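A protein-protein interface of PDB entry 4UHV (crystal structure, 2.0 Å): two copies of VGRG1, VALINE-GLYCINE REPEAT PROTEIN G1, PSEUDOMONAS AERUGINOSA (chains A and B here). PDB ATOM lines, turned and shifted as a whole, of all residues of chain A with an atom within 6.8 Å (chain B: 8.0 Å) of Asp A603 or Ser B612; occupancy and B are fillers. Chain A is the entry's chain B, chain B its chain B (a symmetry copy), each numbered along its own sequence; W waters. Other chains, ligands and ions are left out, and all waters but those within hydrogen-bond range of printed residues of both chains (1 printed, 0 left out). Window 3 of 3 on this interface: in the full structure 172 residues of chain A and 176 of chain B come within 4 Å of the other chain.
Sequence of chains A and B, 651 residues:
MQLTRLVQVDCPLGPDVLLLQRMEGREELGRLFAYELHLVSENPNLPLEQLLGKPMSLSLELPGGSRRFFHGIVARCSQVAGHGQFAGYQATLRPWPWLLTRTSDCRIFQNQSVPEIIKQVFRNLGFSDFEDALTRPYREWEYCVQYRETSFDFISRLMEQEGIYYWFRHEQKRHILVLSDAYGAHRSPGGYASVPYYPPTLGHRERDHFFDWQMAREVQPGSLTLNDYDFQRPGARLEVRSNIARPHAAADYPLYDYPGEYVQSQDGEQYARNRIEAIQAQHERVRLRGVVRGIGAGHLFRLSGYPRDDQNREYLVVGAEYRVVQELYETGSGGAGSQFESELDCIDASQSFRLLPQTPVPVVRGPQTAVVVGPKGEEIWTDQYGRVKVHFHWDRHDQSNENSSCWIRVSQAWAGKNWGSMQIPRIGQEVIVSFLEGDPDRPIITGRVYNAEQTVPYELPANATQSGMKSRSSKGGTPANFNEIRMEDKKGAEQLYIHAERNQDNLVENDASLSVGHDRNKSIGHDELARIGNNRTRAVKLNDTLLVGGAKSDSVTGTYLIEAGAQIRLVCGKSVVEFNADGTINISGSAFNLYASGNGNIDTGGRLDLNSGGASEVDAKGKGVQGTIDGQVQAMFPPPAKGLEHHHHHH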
ATOM      1  N   ASN A 601       6.098  23.790  16.435  1.00  0.00           N
ATOM      2  CA  ASN A 601       5.683  25.095  16.977  1.00  0.00           C
ATOM      3  C   ASN A 601       5.321  25.036  18.461  1.00  0.00           C
ATOM      4  O   ASN A 601       4.585  24.133  18.901  1.00  0.00           O
ATOM      5  CB  ASN A 601       4.475  25.649  16.221  1.00  0.00           C
ATOM      6  CG  ASN A 601       4.711  25.785  14.747  1.00  0.00           C
ATOM      7  OD1 ASN A 601       4.095  25.086  13.939  1.00  0.00           O
ATOM      8  ND2 ASN A 601       5.594  26.690  14.380  1.00  0.00           N
ATOM      9  N   ILE A 602       5.853  25.999  19.212  1.00  0.00           N
ATOM     10  CA  ILE A 602       5.569  26.193  20.630  1.00  0.00           C
ATOM     11  C   ILE A 602       5.156  27.632  20.785  1.00  0.00           C
ATOM     12  O   ILE A 602       5.969  28.525  20.517  1.00  0.00           O
ATOM     13  CB  ILE A 602       6.804  25.969  21.542  1.00  0.00           C
ATOM     14  CG1 ILE A 602       7.694  24.848  21.017  1.00  0.00           C
ATOM     15  CG2 ILE A 602       6.381  25.693  22.979  1.00  0.00           C
ATOM     16  CD1 ILE A 602       8.784  25.356  20.109  1.00  0.00           C
ATOM     17  N   ASP A 603       3.901  27.855  21.208  1.00  0.00           N
ATOM     18  CA  ASP A 603       3.342  29.185  21.328  1.00  0.00           C
ATOM     19  C   ASP A 603       2.572  29.464  22.621  1.00  0.00           C
ATOM     20  O   ASP A 603       2.234  28.561  23.394  1.00  0.00           O
ATOM     21  CB  ASP A 603       2.453  29.476  20.117  1.00  0.00           C
ATOM     22  CG  ASP A 603       3.238  30.043  18.968  1.00  0.00           C
ATOM     23  OD1 ASP A 603       3.510  31.258  19.024  1.00  0.00           O
ATOM     24  OD2 ASP A 603       3.616  29.281  18.051  1.00  0.00           O
ATOM     25  N   THR A 604       2.284  30.744  22.826  1.00  0.00           N
ATOM     26  CA  THR A 604       1.646  31.180  24.046  1.00  0.00           C
ATOM     27  C   THR A 604       0.782  32.404  23.829  1.00  0.00           C
ATOM     28  O   THR A 604       0.631  32.887  22.698  1.00  0.00           O
ATOM     29  CB  THR A 604       2.691  31.480  25.132  1.00  0.00           C
ATOM     30  OG1 THR A 604       2.035  31.712  26.384  1.00  0.00           O
ATOM     31  CG2 THR A 604       3.531  32.696  24.767  1.00  0.00           C
ATOM     32  N   GLY A 605       0.181  32.859  24.924  1.00  0.00           N
ATOM     33  CA  GLY A 605      -0.414  34.184  25.011  1.00  0.00           C
ATOM     34  C   GLY A 605       0.123  34.963  26.191  1.00  0.00           C
ATOM     35  O   GLY A 605      -0.434  36.006  26.549  1.00  0.00           O
ATOM     36  N   GLY A 606       1.173  34.427  26.812  1.00  0.00           N
ATOM     37  CA  GLY A 606       1.951  35.105  27.835  1.00  0.00           C
ATOM     38  C   GLY A 606       3.429  34.969  27.506  1.00  0.00           C
ATOM     39  O   GLY A 606       3.842  35.269  26.391  1.00  0.00           O
ATOM     40  N   LEU A 608       7.212  32.518  27.797  1.00  0.00           N
ATOM     41  CA  LEU A 608       7.678  31.133  27.767  1.00  0.00           C
ATOM     42  C   LEU A 608       9.127  30.990  28.198  1.00  0.00           C
ATOM     43  O   LEU A 608       9.414  30.472  29.289  1.00  0.00           O
ATOM     44  CB  LEU A 608       7.495  30.521  26.369  1.00  0.00           C
ATOM     45  CG  LEU A 608       7.857  29.024  26.279  1.00  0.00           C
ATOM     46  CD1 LEU A 608       6.618  28.156  26.174  1.00  0.00           C
ATOM     47  CD2 LEU A 608       8.781  28.726  25.107  1.00  0.00           C
ATOM     48  N   ILE B 587      -1.607  20.112  20.499  1.00  0.00           N
ATOM     49  CA  ILE B 587      -1.831  20.264  21.923  1.00  0.00           C
ATOM     50  C   ILE B 587      -2.337  21.674  22.155  1.00  0.00           C
ATOM     51  O   ILE B 587      -1.764  22.617  21.631  1.00  0.00           O
ATOM     52  CB  ILE B 587      -0.529  20.087  22.731  1.00  0.00           C
ATOM     53  CG1 ILE B 587       0.381  19.013  22.114  1.00  0.00           C
ATOM     54  CG2 ILE B 587      -0.847  19.818  24.196  1.00  0.00           C
ATOM     55  CD1 ILE B 587       1.854  19.376  22.143  1.00  0.00           C
ATOM     56  N   GLY B 589      -3.925  24.087  25.579  1.00  0.00           N
ATOM     57  CA  GLY B 589      -4.260  24.197  26.995  1.00  0.00           C
ATOM     58  C   GLY B 589      -4.458  25.639  27.418  1.00  0.00           C
ATOM     59  O   GLY B 589      -4.886  26.474  26.617  1.00  0.00           O
ATOM     60  N   ALA B 591      -2.096  26.591  30.285  1.00  0.00           N
ATOM     61  CA  ALA B 591      -0.661  26.631  30.538  1.00  0.00           C
ATOM     62  C   ALA B 591      -0.119  25.227  30.357  1.00  0.00           C
ATOM     63  O   ALA B 591      -0.884  24.249  30.289  1.00  0.00           O
ATOM     64  CB  ALA B 591      -0.360  27.171  31.929  1.00  0.00           C
ATOM     65  N   PHE B 592       1.198  25.115  30.215  1.00  0.00           N
ATOM     66  CA  PHE B 592       1.824  23.812  30.276  1.00  0.00           C
ATOM     67  C   PHE B 592       3.114  23.854  31.101  1.00  0.00           C
ATOM     68  O   PHE B 592       3.798  24.900  31.187  1.00  0.00           O
ATOM     69  CB  PHE B 592       2.042  23.237  28.859  1.00  0.00           C
ATOM     70  CG  PHE B 592       2.952  24.057  28.002  1.00  0.00           C
ATOM     71  CD1 PHE B 592       2.531  25.267  27.494  1.00  0.00           C
ATOM     72  CD2 PHE B 592       4.218  23.615  27.696  1.00  0.00           C
ATOM     73  CE1 PHE B 592       3.364  26.043  26.717  1.00  0.00           C
ATOM     74  CE2 PHE B 592       5.060  24.372  26.915  1.00  0.00           C
ATOM     75  CZ  PHE B 592       4.635  25.583  26.416  1.00  0.00           C
ATOM     76  N   LEU B 608      12.173  25.002  13.852  1.00  0.00           N
ATOM     77  CA  LEU B 608      11.444  25.017  15.119  1.00  0.00           C
ATOM     78  C   LEU B 608      11.321  26.411  15.709  1.00  0.00           C
ATOM     79  O   LEU B 608      10.227  26.998  15.719  1.00  0.00           O
ATOM     80  CB  LEU B 608      12.104  24.081  16.145  1.00  0.00           C
ATOM     81  CG  LEU B 608      11.331  23.952  17.474  1.00  0.00           C
ATOM     82  CD1 LEU B 608      10.630  22.611  17.583  1.00  0.00           C
ATOM     83  CD2 LEU B 608      12.233  24.149  18.683  1.00  0.00           C
ATOM     84  N   ASP B 609      12.457  26.912  16.205  1.00  0.00           N
ATOM     85  CA  ASP B 609      12.559  28.136  17.011  1.00  0.00           C
ATOM     86  C   ASP B 609      11.579  28.181  18.192  1.00  0.00           C
ATOM     87  O   ASP B 609      11.568  27.270  19.020  1.00  0.00           O
ATOM     88  CB  ASP B 609      12.456  29.369  16.111  1.00  0.00           C
ATOM     89  CG  ASP B 609      13.634  29.495  15.163  1.00  0.00           C
ATOM     90  OD1 ASP B 609      13.863  28.564  14.368  1.00  0.00           O
ATOM     91  OD2 ASP B 609      14.332  30.528  15.223  1.00  0.00           O
ATOM     92  N   LEU B 610      10.766  29.234  18.279  1.00  0.00           N
ATOM     93  CA  LEU B 610       9.829  29.410  19.381  1.00  0.00           C
ATOM     94  C   LEU B 610       8.802  30.464  18.964  1.00  0.00           C
ATOM     95  O   LEU B 610       9.136  31.415  18.265  1.00  0.00           O
ATOM     96  CB  LEU B 610      10.607  29.780  20.662  1.00  0.00           C
ATOM     97  CG  LEU B 610      10.305  31.028  21.511  1.00  0.00           C
ATOM     98  CD1 LEU B 610       9.073  30.854  22.373  1.00  0.00           C
ATOM     99  CD2 LEU B 610      11.501  31.396  22.386  1.00  0.00           C
ATOM    100  N   ASN B 611       7.545  30.270  19.347  1.00  0.00           N
ATOM    101  CA  ASN B 611       6.481  31.259  19.106  1.00  0.00           C
ATOM    102  C   ASN B 611       6.050  31.467  17.641  1.00  0.00           C
ATOM    103  O   ASN B 611       6.674  30.964  16.713  1.00  0.00           O
ATOM    104  CB  ASN B 611       6.816  32.610  19.784  1.00  0.00           C
ATOM    105  CG  ASN B 611       7.618  33.545  18.890  1.00  0.00           C
ATOM    106  OD1 ASN B 611       7.065  34.211  18.012  1.00  0.00           O
ATOM    107  ND2 ASN B 611       8.928  33.603  19.115  1.00  0.00           N
ATOM    108  N   SER B 612       4.964  32.230  17.487  1.00  0.00           N
ATOM    109  CA  SER B 612       4.199  32.454  16.241  1.00  0.00           C
ATOM    110  C   SER B 612       3.300  31.297  15.755  1.00  0.00           C
ATOM    111  O   SER B 612       2.116  31.520  15.541  1.00  0.00           O
ATOM    112  CB  SER B 612       5.033  33.070  15.083  1.00  0.00           C
ATOM    113  OG  SER B 612       6.313  32.491  14.912  1.00  0.00           O
ATOM    114  N   GLY B 613       3.829  30.079  15.624  1.00  0.00           N
ATOM    115  CA  GLY B 613       3.209  29.021  14.789  1.00  0.00           C
ATOM    116  C   GLY B 613       1.952  28.220  15.178  1.00  0.00           C
ATOM    117  O   GLY B 613       0.985  28.188  14.418  1.00  0.00           O
ATOM    118  N   GLY B 614       1.952  27.544  16.323  1.00  0.00           N
ATOM    119  CA  GLY B 614       0.823  26.684  16.682  1.00  0.00           C
ATOM    120  C   GLY B 614      -0.436  27.512  16.779  1.00  0.00           C
ATOM    121  O   GLY B 614      -0.374  28.692  17.124  1.00  0.00           O
ATOM    122  N   ALA B 615      -1.577  26.894  16.484  1.00  0.00           N
ATOM    123  CA  ALA B 615      -2.811  27.647  16.199  1.00  0.00           C
ATOM    124  C   ALA B 615      -3.180  28.615  17.306  1.00  0.00           C
ATOM    125  O   ALA B 615      -2.761  28.450  18.444  1.00  0.00           O
ATOM    126  CB  ALA B 615      -3.971  26.701  15.948  1.00  0.00           C
ATOM    127  N   SER B 616      -3.961  29.625  16.952  1.00  0.00           N
ATOM    128  CA  SER B 616      -4.437  30.591  17.935  1.00  0.00           C
ATOM    129  C   SER B 616      -5.322  29.852  18.917  1.00  0.00           C
ATOM    130  O   SER B 616      -5.227  30.068  20.106  1.00  0.00           O
ATOM    131  CB  SER B 616      -5.169  31.755  17.268  1.00  0.00           C
ATOM    132  OG  SER B 616      -5.626  32.689  18.234  1.00  0.00           O
HETATM  133  O   HOH W   1       3.020  26.571  18.726  1.00  0.00           O
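Position printed for both chains: 608. Of the 13 pairs that touch across the chains among the printed residues, none has its exchanged pair printed and touching as well.
Of the printed residues of chain B, Asp A603 touches Asn B611, Ser B612, Gly B613 and Gly B614. Ser B612 touches just one residue of chain A: Asp A603 (2.3 Å). Of the printed residues of chain A, Gly B614 touches Asn A601 (3.2 Å) and Asp A603 (3.0 Å). Printed residues of chain B within 4 Å of Leu A608: Phe B592 and Leu B610. The nearest residue of chain B that does not touch Asp A603 is Phe B592 (4.3 Å). The nearest residue of chain A that does not touch Ser B612 is Ile A602 (4.9 Å). The nearest printed residue of chain B that does not touch Ile A602 is Ser B612 (4.9 Å).
Water W1 lies within hydrogen-bond range of the backbone NH (N) of Gly B614 (2.8 Å), the side-chain carboxylate (OD2) of Asp A603 (2.9 Å), the backbone carbonyl oxygen (O) of Asn A601 (2.9 Å) and the backbone NH (N) of Ile A602 (2.9 Å).
N of Gly B614 lies within hydrogen-bond range of OD2 of Asp A603, at 3.0 Å. OD2 of Asp A603 lies within hydrogen-bond range of N of Gly B613 (2.6 Å). N of Asn B611 lies within hydrogen-bond range of O of Ile A602 (2.6 Å). OD2 of Asp A603 lies close to N of Ser B612 (3.3 Å).
Hydrophobic or aromatic side chains of chain B that line the printed part of chain A: Phe B592, Leu B608 and Leu B610. Of the 7 printed residues of chain A, 4 touch a printed residue of chain B. Hydrophobic or aromatic side chains of chain A within 4 Å of the printed part of chain B: Ile A602 and Leu A608. Among the printed residues, no Asp or Glu carboxylate lies within 4 Å of a Lys or Arg side-chain nitrogen of the other chain.
Among the printed residues, pairs that only touch across the chains: Asp A603 with Asn B611 (2.9 Å), Asn A601 with Gly B614 (3.2 Å), Leu A608 with Phe B592 (3.3 Å), Asn A601 with Gly B613 (3.4 Å), Leu A608 with Leu B610 (3.5 Å), Ile A602 with Asp B609 (3.5 Å), Ile A602 with Leu B610 (3.8 Å), Ile A602 with Phe B592 (3.9 Å) and Ile A602 with Leu B608 (3.9 Å).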
